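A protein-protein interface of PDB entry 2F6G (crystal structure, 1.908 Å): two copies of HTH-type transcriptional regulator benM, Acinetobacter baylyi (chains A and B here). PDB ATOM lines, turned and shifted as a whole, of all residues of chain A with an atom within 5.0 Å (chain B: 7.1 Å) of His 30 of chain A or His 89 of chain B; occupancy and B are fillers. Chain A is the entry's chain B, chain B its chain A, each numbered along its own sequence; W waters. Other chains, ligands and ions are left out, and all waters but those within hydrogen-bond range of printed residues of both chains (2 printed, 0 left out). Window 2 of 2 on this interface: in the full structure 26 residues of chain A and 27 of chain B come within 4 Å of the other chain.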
ATOM      1  N   LEU A  25      15.494   4.987  12.855  1.00  0.00           N
ATOM      2  CA  LEU A  25      16.442   5.757  12.026  1.00  0.00           C
ATOM      3  C   LEU A  25      17.899   5.324  12.214  1.00  0.00           C
ATOM      4  O   LEU A  25      18.596   5.080  11.226  1.00  0.00           O
ATOM      5  CB  LEU A  25      16.316   7.270  12.269  1.00  0.00           C
ATOM      6  CG  LEU A  25      16.525   8.252  11.103  1.00  0.00           C
ATOM      7  CD1 LEU A  25      16.994   9.597  11.618  1.00  0.00           C
ATOM      8  CD2 LEU A  25      17.472   7.758  10.023  1.00  0.00           C
ATOM      9  N   PRO A  26      18.383   5.256  13.473  1.00  0.00           N
ATOM     10  CA  PRO A  26      19.771   4.831  13.686  1.00  0.00           C
ATOM     11  C   PRO A  26      20.163   3.497  13.036  1.00  0.00           C
ATOM     12  O   PRO A  26      21.259   3.396  12.471  1.00  0.00           O
ATOM     13  CB  PRO A  26      19.874   4.746  15.211  1.00  0.00           C
ATOM     14  CG  PRO A  26      18.891   5.744  15.681  1.00  0.00           C
ATOM     15  CD  PRO A  26      17.736   5.603  14.752  1.00  0.00           C
ATOM     16  N   ARG A  27      19.306   2.481  13.112  1.00  0.00           N
ATOM     17  CA  ARG A  27      19.655   1.185  12.511  1.00  0.00           C
ATOM     18  C   ARG A  27      19.608   1.278  10.986  1.00  0.00           C
ATOM     19  O   ARG A  27      20.377   0.611  10.312  1.00  0.00           O
ATOM     20  CB  ARG A  27      18.797   0.031  13.062  1.00  0.00           C
ATOM     21  CG  ARG A  27      17.392  -0.096  12.491  1.00  0.00           C
ATOM     22  CD  ARG A  27      16.587  -1.166  13.225  1.00  0.00           C
ATOM     23  NE  ARG A  27      16.136  -0.704  14.536  1.00  0.00           N
ATOM     24  CZ  ARG A  27      15.196  -1.293  15.270  1.00  0.00           C
ATOM     25  NH1 ARG A  27      14.854  -0.771  16.440  1.00  0.00           N
ATOM     26  NH2 ARG A  27      14.600  -2.394  14.857  1.00  0.00           N
ATOM     27  N   ILE A  28      18.739   2.138  10.451  1.00  0.00           N
ATOM     28  CA  ILE A  28      18.716   2.411   9.003  1.00  0.00           C
ATOM     29  C   ILE A  28      20.037   3.053   8.554  1.00  0.00           C
ATOM     30  O   ILE A  28      20.638   2.613   7.583  1.00  0.00           O
ATOM     31  CB  ILE A  28      17.492   3.278   8.590  1.00  0.00           C
ATOM     32  CG1 ILE A  28      16.200   2.463   8.720  1.00  0.00           C
ATOM     33  CG2 ILE A  28      17.641   3.808   7.145  1.00  0.00           C
ATOM     34  CD1 ILE A  28      14.937   3.304   8.768  1.00  0.00           C
ATOM     35  N   ILE A  29      20.510   4.064   9.278  1.00  0.00           N
ATOM     36  CA  ILE A  29      21.791   4.685   8.956  1.00  0.00           C
ATOM     37  C   ILE A  29      22.959   3.719   9.131  1.00  0.00           C
ATOM     38  O   ILE A  29      23.880   3.701   8.306  1.00  0.00           O
ATOM     39  CB  ILE A  29      22.060   5.944   9.813  1.00  0.00           C
ATOM     40  CG1 ILE A  29      20.996   7.007   9.533  1.00  0.00           C
ATOM     41  CG2 ILE A  29      23.472   6.475   9.563  1.00  0.00           C
ATOM     42  CD1 ILE A  29      20.833   7.362   8.059  1.00  0.00           C
ATOM     43  N   HIS A  30      22.936   2.924  10.196  1.00  0.00           N
ATOM     44  CA  HIS A  30      24.021   1.975  10.434  1.00  0.00           C
ATOM     45  C   HIS A  30      24.141   0.956   9.288  1.00  0.00           C
ATOM     46  O   HIS A  30      25.236   0.670   8.817  1.00  0.00           O
ATOM     47  CB  HIS A  30      23.828   1.250  11.768  1.00  0.00           C
ATOM     48  CG  HIS A  30      24.991   0.395  12.153  1.00  0.00           C
ATOM     49  ND1 HIS A  30      25.133  -0.901  11.714  1.00  0.00           N
ATOM     50  CD2 HIS A  30      26.067   0.647  12.935  1.00  0.00           C
ATOM     51  CE1 HIS A  30      26.247  -1.413  12.206  1.00  0.00           C
ATOM     52  NE2 HIS A  30      26.831  -0.492  12.952  1.00  0.00           N
ATOM     53  N   LEU A  31      23.010   0.420   8.850  1.00  0.00           N
ATOM     54  CA  LEU A  31      22.983  -0.548   7.753  1.00  0.00           C
ATOM     55  C   LEU A  31      23.387   0.086   6.423  1.00  0.00           C
ATOM     56  O   LEU A  31      24.138  -0.501   5.642  1.00  0.00           O
ATOM     57  CB  LEU A  31      21.587  -1.159   7.638  1.00  0.00           C
ATOM     58  CG  LEU A  31      21.405  -2.199   6.530  1.00  0.00           C
ATOM     59  CD1 LEU A  31      22.456  -3.297   6.658  1.00  0.00           C
ATOM     60  CD2 LEU A  31      19.991  -2.776   6.558  1.00  0.00           C
ATOM     61  N   TYR A  32      22.868   1.281   6.171  1.00  0.00           N
ATOM     62  CA  TYR A  32      23.263   2.088   5.018  1.00  0.00           C
ATOM     63  C   TYR A  32      24.784   2.318   4.986  1.00  0.00           C
ATOM     64  O   TYR A  32      25.419   2.150   3.942  1.00  0.00           O
ATOM     65  CB  TYR A  32      22.487   3.411   5.059  1.00  0.00           C
ATOM     66  CG  TYR A  32      22.708   4.335   3.887  1.00  0.00           C
ATOM     67  CD1 TYR A  32      22.386   3.944   2.592  1.00  0.00           C
ATOM     68  CD2 TYR A  32      23.214   5.617   4.080  1.00  0.00           C
ATOM     69  CE1 TYR A  32      22.583   4.795   1.521  1.00  0.00           C
ATOM     70  CE2 TYR A  32      23.414   6.473   3.011  1.00  0.00           C
ATOM     71  CZ  TYR A  32      23.095   6.057   1.736  1.00  0.00           C
ATOM     72  OH  TYR A  32      23.286   6.906   0.678  1.00  0.00           O
ATOM     73  N   ARG A  33      25.364   2.696   6.127  1.00  0.00           N
ATOM     74  CA  ARG A  33      26.818   2.863   6.250  1.00  0.00           C
ATOM     75  C   ARG A  33      27.548   1.554   5.980  1.00  0.00           C
ATOM     76  O   ARG A  33      28.546   1.522   5.258  1.00  0.00           O
ATOM     77  CB  ARG A  33      27.203   3.346   7.651  1.00  0.00           C
ATOM     78  CG  ARG A  33      27.099   4.842   7.859  1.00  0.00           C
ATOM     79  CD  ARG A  33      27.816   5.261   9.136  1.00  0.00           C
ATOM     80  NE  ARG A  33      27.928   6.718   9.249  1.00  0.00           N
ATOM     81  CZ  ARG A  33      27.301   7.482  10.140  1.00  0.00           C
ATOM     82  NH1 ARG A  33      26.486   6.962  11.048  1.00  0.00           N
ATOM     83  NH2 ARG A  33      27.499   8.794  10.124  1.00  0.00           N
ATOM     84  N   GLN A  34      27.046   0.476   6.575  1.00  0.00           N
ATOM     85  CA  GLN A  34      27.651  -0.845   6.428  1.00  0.00           C
ATOM     86  C   GLN A  34      27.629  -1.306   4.971  1.00  0.00           C
ATOM     87  O   GLN A  34      28.609  -1.870   4.483  1.00  0.00           O
ATOM     88  CB  GLN A  34      26.921  -1.855   7.312  1.00  0.00           C
ATOM     89  CG  GLN A  34      27.544  -3.236   7.336  1.00  0.00           C
ATOM     90  CD  GLN A  34      26.764  -4.211   8.195  1.00  0.00           C
ATOM     91  OE1 GLN A  34      26.417  -3.910   9.337  1.00  0.00           O
ATOM     92  NE2 GLN A  34      26.489  -5.389   7.650  1.00  0.00           N
ATOM     93  N   ALA B  87      28.809   4.422  26.376  1.00  0.00           N
ATOM     94  CA  ALA B  87      27.811   3.976  25.410  1.00  0.00           C
ATOM     95  C   ALA B  87      28.526   3.571  24.126  1.00  0.00           C
ATOM     96  O   ALA B  87      29.304   4.348  23.576  1.00  0.00           O
ATOM     97  CB  ALA B  87      26.791   5.079  25.131  1.00  0.00           C
ATOM     98  N   VAL B  88      28.278   2.344  23.677  1.00  0.00           N
ATOM     99  CA  VAL B  88      28.914   1.797  22.473  1.00  0.00           C
ATOM    100  C   VAL B  88      27.890   1.036  21.636  1.00  0.00           C
ATOM    101  O   VAL B  88      26.850   0.609  22.148  1.00  0.00           O
ATOM    102  CB  VAL B  88      30.088   0.827  22.827  1.00  0.00           C
ATOM    103  CG1 VAL B  88      31.174   1.547  23.632  1.00  0.00           C
ATOM    104  CG2 VAL B  88      29.592  -0.385  23.599  1.00  0.00           C
ATOM    105  N   HIS B  89      28.186   0.861  20.352  1.00  0.00           N
ATOM    106  CA  HIS B  89      27.397  -0.043  19.515  1.00  0.00           C
ATOM    107  C   HIS B  89      27.631  -1.475  20.001  1.00  0.00           C
ATOM    108  O   HIS B  89      28.715  -1.802  20.478  1.00  0.00           O
ATOM    109  CB  HIS B  89      27.807   0.075  18.042  1.00  0.00           C
ATOM    110  CG  HIS B  89      26.828  -0.545  17.092  1.00  0.00           C
ATOM    111  ND1 HIS B  89      25.703   0.115  16.653  1.00  0.00           N
ATOM    112  CD2 HIS B  89      26.806  -1.760  16.494  1.00  0.00           C
ATOM    113  CE1 HIS B  89      25.023  -0.667  15.836  1.00  0.00           C
ATOM    114  NE2 HIS B  89      25.675  -1.808  15.716  1.00  0.00           N
ATOM    115  N   ALA B  90      26.620  -2.324  19.867  1.00  0.00           N
ATOM    116  CA  ALA B  90      26.700  -3.722  20.313  1.00  0.00           C
ATOM    117  C   ALA B  90      27.936  -4.469  19.790  1.00  0.00           C
ATOM    118  O   ALA B  90      28.532  -5.273  20.504  1.00  0.00           O
ATOM    119  CB  ALA B  90      25.439  -4.457  19.916  1.00  0.00           C
ATOM    120  N   SER B  91      28.320  -4.174  18.551  1.00  0.00           N
ATOM    121  CA  SER B  91      29.443  -4.830  17.878  1.00  0.00           C
ATOM    122  C   SER B  91      30.826  -4.279  18.238  1.00  0.00           C
ATOM    123  O   SER B  91      31.835  -4.849  17.837  1.00  0.00           O
ATOM    124  CB  SER B  91      29.262  -4.720  16.357  1.00  0.00           C
ATOM    125  OG  SER B  91      29.403  -3.369  15.933  1.00  0.00           O
ATOM    126  N   HIS B  92      30.885  -3.179  18.982  1.00  0.00           N
ATOM    127  CA  HIS B  92      32.166  -2.537  19.284  1.00  0.00           C
ATOM    128  C   HIS B  92      33.055  -3.437  20.155  1.00  0.00           C
ATOM    129  O   HIS B  92      32.552  -4.101  21.061  1.00  0.00           O
ATOM    130  CB  HIS B  92      31.922  -1.194  19.978  1.00  0.00           C
ATOM    131  CG  HIS B  92      33.063  -0.237  19.858  1.00  0.00           C
ATOM    132  ND1 HIS B  92      34.152  -0.274  20.696  1.00  0.00           N
ATOM    133  CD2 HIS B  92      33.285   0.785  18.999  1.00  0.00           C
ATOM    134  CE1 HIS B  92      35.006   0.674  20.354  1.00  0.00           C
ATOM    135  NE2 HIS B  92      34.502   1.331  19.325  1.00  0.00           N
ATOM    136  N   PRO B  93      34.378  -3.487  19.867  1.00  0.00           N
ATOM    137  CA  PRO B  93      35.335  -4.239  20.696  1.00  0.00           C
ATOM    138  C   PRO B  93      35.231  -3.994  22.212  1.00  0.00           C
ATOM    139  O   PRO B  93      35.381  -4.928  22.995  1.00  0.00           O
ATOM    140  CB  PRO B  93      36.700  -3.759  20.177  1.00  0.00           C
ATOM    141  CG  PRO B  93      36.448  -3.407  18.756  1.00  0.00           C
ATOM    142  CD  PRO B  93      35.047  -2.857  18.708  1.00  0.00           C
ATOM    143  N   LEU B  94      34.988  -2.750  22.614  1.00  0.00           N
ATOM    144  CA  LEU B  94      34.799  -2.401  24.027  1.00  0.00           C
ATOM    145  C   LEU B  94      33.610  -3.115  24.660  1.00  0.00           C
ATOM    146  O   LEU B  94      33.604  -3.362  25.868  1.00  0.00           O
ATOM    147  CB  LEU B  94      34.623  -0.890  24.194  1.00  0.00           C
ATOM    148  CG  LEU B  94      35.842  -0.002  23.928  1.00  0.00           C
ATOM    149  CD1 LEU B  94      35.418   1.455  23.892  1.00  0.00           C
ATOM    150  CD2 LEU B  94      36.911  -0.220  24.985  1.00  0.00           C
ATOM    151  N   ASN B  95      32.607  -3.449  23.843  1.00  0.00           N
ATOM    152  CA  ASN B  95      31.446  -4.198  24.323  1.00  0.00           C
ATOM    153  C   ASN B  95      31.772  -5.656  24.671  1.00  0.00           C
ATOM    154  O   ASN B  95      30.990  -6.312  25.352  1.00  0.00           O
ATOM    155  CB  ASN B  95      30.294  -4.124  23.312  1.00  0.00           C
ATOM    156  CG  ASN B  95      28.938  -4.432  23.933  1.00  0.00           C
ATOM    157  OD1 ASN B  95      28.055  -4.976  23.274  1.00  0.00           O
ATOM    158  ND2 ASN B  95      28.765  -4.082  25.198  1.00  0.00           N
ATOM    159  N   LEU B 153      23.754   8.765  17.627  1.00  0.00           N
ATOM    160  CA  LEU B 153      24.917   8.699  16.746  1.00  0.00           C
ATOM    161  C   LEU B 153      25.754   7.455  17.010  1.00  0.00           C
ATOM    162  O   LEU B 153      26.265   6.844  16.072  1.00  0.00           O
ATOM    163  CB  LEU B 153      25.784   9.962  16.871  1.00  0.00           C
ATOM    164  CG  LEU B 153      25.164  11.246  16.318  1.00  0.00           C
ATOM    165  CD1 LEU B 153      25.998  12.444  16.734  1.00  0.00           C
ATOM    166  CD2 LEU B 153      25.026  11.186  14.792  1.00  0.00           C
ATOM    167  N   VAL B 154      25.877   7.082  18.282  1.00  0.00           N
ATOM    168  CA  VAL B 154      26.531   5.840  18.681  1.00  0.00           C
ATOM    169  C   VAL B 154      25.793   4.652  18.064  1.00  0.00           C
ATOM    170  O   VAL B 154      26.410   3.776  17.456  1.00  0.00           O
ATOM    171  CB  VAL B 154      26.557   5.676  20.224  1.00  0.00           C
ATOM    172  CG1 VAL B 154      27.004   4.270  20.620  1.00  0.00           C
ATOM    173  CG2 VAL B 154      27.469   6.732  20.875  1.00  0.00           C
ATOM    174  N   ALA B 155      24.468   4.636  18.216  1.00  0.00           N
ATOM    175  CA  ALA B 155      23.640   3.551  17.676  1.00  0.00           C
ATOM    176  C   ALA B 155      23.737   3.472  16.158  1.00  0.00           C
ATOM    177  O   ALA B 155      23.692   2.379  15.583  1.00  0.00           O
ATOM    178  CB  ALA B 155      22.192   3.724  18.106  1.00  0.00           C
ATOM    179  N   ALA B 156      23.865   4.627  15.512  1.00  0.00           N
ATOM    180  CA  ALA B 156      24.071   4.691  14.059  1.00  0.00           C
ATOM    181  C   ALA B 156      25.505   4.351  13.635  1.00  0.00           C
ATOM    182  O   ALA B 156      25.781   4.202  12.444  1.00  0.00           O
ATOM    183  CB  ALA B 156      23.659   6.058  13.516  1.00  0.00           C
ATOM    184  N   GLY B 157      26.406   4.232  14.606  1.00  0.00           N
ATOM    185  CA  GLY B 157      27.745   3.682  14.386  1.00  0.00           C
ATOM    186  C   GLY B 157      28.843   4.715  14.245  1.00  0.00           C
ATOM    187  O   GLY B 157      29.888   4.425  13.673  1.00  0.00           O
ATOM    188  N   GLU B 158      28.621   5.908  14.788  1.00  0.00           N
ATOM    189  CA  GLU B 158      29.529   7.037  14.576  1.00  0.00           C
ATOM    190  C   GLU B 158      30.587   7.189  15.674  1.00  0.00           C
ATOM    191  O   GLU B 158      31.508   8.000  15.536  1.00  0.00           O
ATOM    192  CB  GLU B 158      28.728   8.338  14.472  1.00  0.00           C
ATOM    193  CG  GLU B 158      29.130   9.225  13.307  1.00  0.00           C
ATOM    194  CD  GLU B 158      28.420  10.567  13.336  1.00  0.00           C
ATOM    195  OE1 GLU B 158      28.638  11.327  14.307  1.00  0.00           O
ATOM    196  OE2 GLU B 158      27.647  10.853  12.396  1.00  0.00           O
ATOM    197  N   GLY B 159      30.462   6.440  16.764  1.00  0.00           N
ATOM    198  CA  GLY B 159      31.456   6.509  17.833  1.00  0.00           C
ATOM    199  C   GLY B 159      30.984   5.948  19.156  1.00  0.00           C
ATOM    200  O   GLY B 159      30.129   5.065  19.196  1.00  0.00           O
ATOM    201  N   ILE B 160      31.575   6.457  20.234  1.00  0.00           N
ATOM    202  CA  ILE B 160      31.200   6.097  21.599  1.00  0.00           C
ATOM    203  C   ILE B 160      30.906   7.370  22.367  1.00  0.00           C
ATOM    204  O   ILE B 160      31.238   8.459  21.913  1.00  0.00           O
ATOM    205  CB  ILE B 160      32.321   5.311  22.313  1.00  0.00           C
ATOM    206  CG1 ILE B 160      33.535   6.213  22.617  1.00  0.00           C
ATOM    207  CG2 ILE B 160      32.740   4.118  21.459  1.00  0.00           C
ATOM    208  CD1 ILE B 160      34.615   5.538  23.432  1.00  0.00           C
ATOM    209  N   PHE B 173      18.062   0.292  20.094  1.00  0.00           N
ATOM    210  CA  PHE B 173      18.431  -0.919  19.367  1.00  0.00           C
ATOM    211  C   PHE B 173      19.930  -0.928  19.087  1.00  0.00           C
ATOM    212  O   PHE B 173      20.467   0.025  18.518  1.00  0.00           O
ATOM    213  CB  PHE B 173      17.628  -0.975  18.067  1.00  0.00           C
ATOM    214  CG  PHE B 173      17.936  -2.145  17.189  1.00  0.00           C
ATOM    215  CD1 PHE B 173      17.250  -3.340  17.336  1.00  0.00           C
ATOM    216  CD2 PHE B 173      18.878  -2.037  16.173  1.00  0.00           C
ATOM    217  CE1 PHE B 173      17.516  -4.420  16.496  1.00  0.00           C
ATOM    218  CE2 PHE B 173      19.148  -3.102  15.339  1.00  0.00           C
ATOM    219  CZ  PHE B 173      18.473  -4.297  15.502  1.00  0.00           C
ATOM    220  N   ASN B 174      20.593  -2.007  19.510  1.00  0.00           N
ATOM    221  CA  ASN B 174      22.039  -2.195  19.335  1.00  0.00           C
ATOM    222  C   ASN B 174      22.928  -1.143  20.016  1.00  0.00           C
ATOM    223  O   ASN B 174      24.069  -0.903  19.591  1.00  0.00           O
ATOM    224  CB  ASN B 174      22.385  -2.352  17.850  1.00  0.00           C
ATOM    225  CG  ASN B 174      22.296  -3.793  17.379  1.00  0.00           C
ATOM    226  OD1 ASN B 174      22.289  -4.728  18.185  1.00  0.00           O
ATOM    227  ND2 ASN B 174      22.267  -3.982  16.067  1.00  0.00           N
ATOM    228  N   LEU B 175      22.412  -0.571  21.105  1.00  0.00           N
ATOM    229  CA  LEU B 175      23.172   0.321  21.969  1.00  0.00           C
ATOM    230  C   LEU B 175      23.416  -0.375  23.306  1.00  0.00           C
ATOM    231  O   LEU B 175      22.470  -0.836  23.957  1.00  0.00           O
ATOM    232  CB  LEU B 175      22.402   1.616  22.188  1.00  0.00           C
ATOM    233  CG  LEU B 175      22.981   2.627  23.178  1.00  0.00           C
ATOM    234  CD1 LEU B 175      24.283   3.194  22.666  1.00  0.00           C
ATOM    235  CD2 LEU B 175      21.966   3.738  23.406  1.00  0.00           C
ATOM    236  N   SER B 176      24.684  -0.442  23.702  1.00  0.00           N
ATOM    237  CA  SER B 176      25.104  -1.139  24.913  1.00  0.00           C
ATOM    238  C   SER B 176      25.903  -0.194  25.808  1.00  0.00           C
ATOM    239  O   SER B 176      26.622   0.668  25.310  1.00  0.00           O
ATOM    240  CB  SER B 176      25.955  -2.341  24.526  1.00  0.00           C
ATOM    241  OG  SER B 176      26.432  -3.025  25.662  1.00  0.00           O
ATOM    242  N   VAL B 178      28.742   0.157  28.834  1.00  0.00           N
ATOM    243  CA  VAL B 178      29.865  -0.561  29.432  1.00  0.00           C
ATOM    244  C   VAL B 178      30.338   0.173  30.693  1.00  0.00           C
ATOM    245  O   VAL B 178      30.561   1.391  30.659  1.00  0.00           O
ATOM    246  CB  VAL B 178      31.029  -0.717  28.417  1.00  0.00           C
ATOM    247  CG1 VAL B 178      32.190  -1.472  29.029  1.00  0.00           C
ATOM    248  CG2 VAL B 178      30.542  -1.438  27.154  1.00  0.00           C
HETATM  249  O   HOH W   1      25.698   8.365  13.663  1.00  0.00           O
HETATM  250  O   HOH W   2      21.313   0.934  15.412  1.00  0.00           O
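Hydrophobic or aromatic side chains of chain B that line the printed part of chain A: His 89, Ala 155, Ala 156 and Phe 173.
Along chain A the printed residues that touch a printed residue of chain B span positions 26 to 33.
Among the printed residues, 10 pairs touch across the chains.
A ring nitrogen (ND1) of His 89 of chain B is in hydrogen-bond range of the backbone carbonyl oxygen (O) of Ala 155 of chain B, at 3.2 Å.
N of Glu 158 of chain B lies within hydrogen-bond range of O of Leu 153 of chain B (2.8 Å).
Water W2 lies within hydrogen-bond range of the backbone carbonyl oxygen (O) of Ala 155 of chain B (2.8 Å), the backbone carbonyl oxygen (O) of Phe 173 of chain B (3.3 Å) and the backbone NH (N) of Arg 27 of chain A (3.4 Å).
Water W1 lies within hydrogen-bond range of the backbone carbonyl oxygen of Leu 153 of chain B (2.9 Å), the guanidinium group of Arg 33 of chain A (3.1 Å) and the side-chain carboxylate of Glu 158 of chain B (3.4 Å).
No position is printed for both chains.
Pro 26 of chain A touches Ala 155 of chain B (CB to CB, 3.8 Å).
O of Pro 26 of chain A touches CA of Ala 156 of chain B (3.5 Å).
Phe 173 of chain B touches Arg 27 of chain A.
CG2 of Ile 29 of chain A touches CB of Ala 156 of chain B, at 3.98 Å.
His 30 of chain A touches Ala 155 of chain B (CD2 to O, 3.96 Å).
His 30 of chain A touches Ala 156 of chain B.
CD2 of His 30 of chain A touches CA of Gly 157 of chain B, at 3.8 Å.
NE2 of His 89 of chain B sits at hydrogen-bond distance from NE2 of His 30 of chain A (3.3 Å).
O of Ala 156 of chain B lies within hydrogen-bond range of NH1 of Arg 33 of chain A, 3.2 Å away.
The side-chain carboxylate (OE2) of Glu 158 of chain B lies within salt-bridge range of the guanidinium group (NH2) of Arg 33 of chain A (3.1 Å).
Of chain B, only His 89 (3.3 Å), Ala 155 (3.96 Å), Ala 156 (3.5 Å) and Gly 157 (3.8 Å) come within 4 Å of His 30 of chain A.
Of the printed residues of chain A, His 89 of chain B touches His 30.
Printed residues of chain A within 4 Å of Gly 157 of chain B: His 30 (3.8 Å).
Of the printed residues of chain B, Ile 29 of chain A touches Ala 156.
Of the printed residues of chain A, Ala 155 of chain B touches Pro 26 (3.8 Å) and His 30 (3.96 Å).
Ala 90 of chain B touches none of the printed residues of chain A.
The nearest printed residue of chain A that does not touch Gly 157 of chain B is Arg 33 of chain A (4.5 Å).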
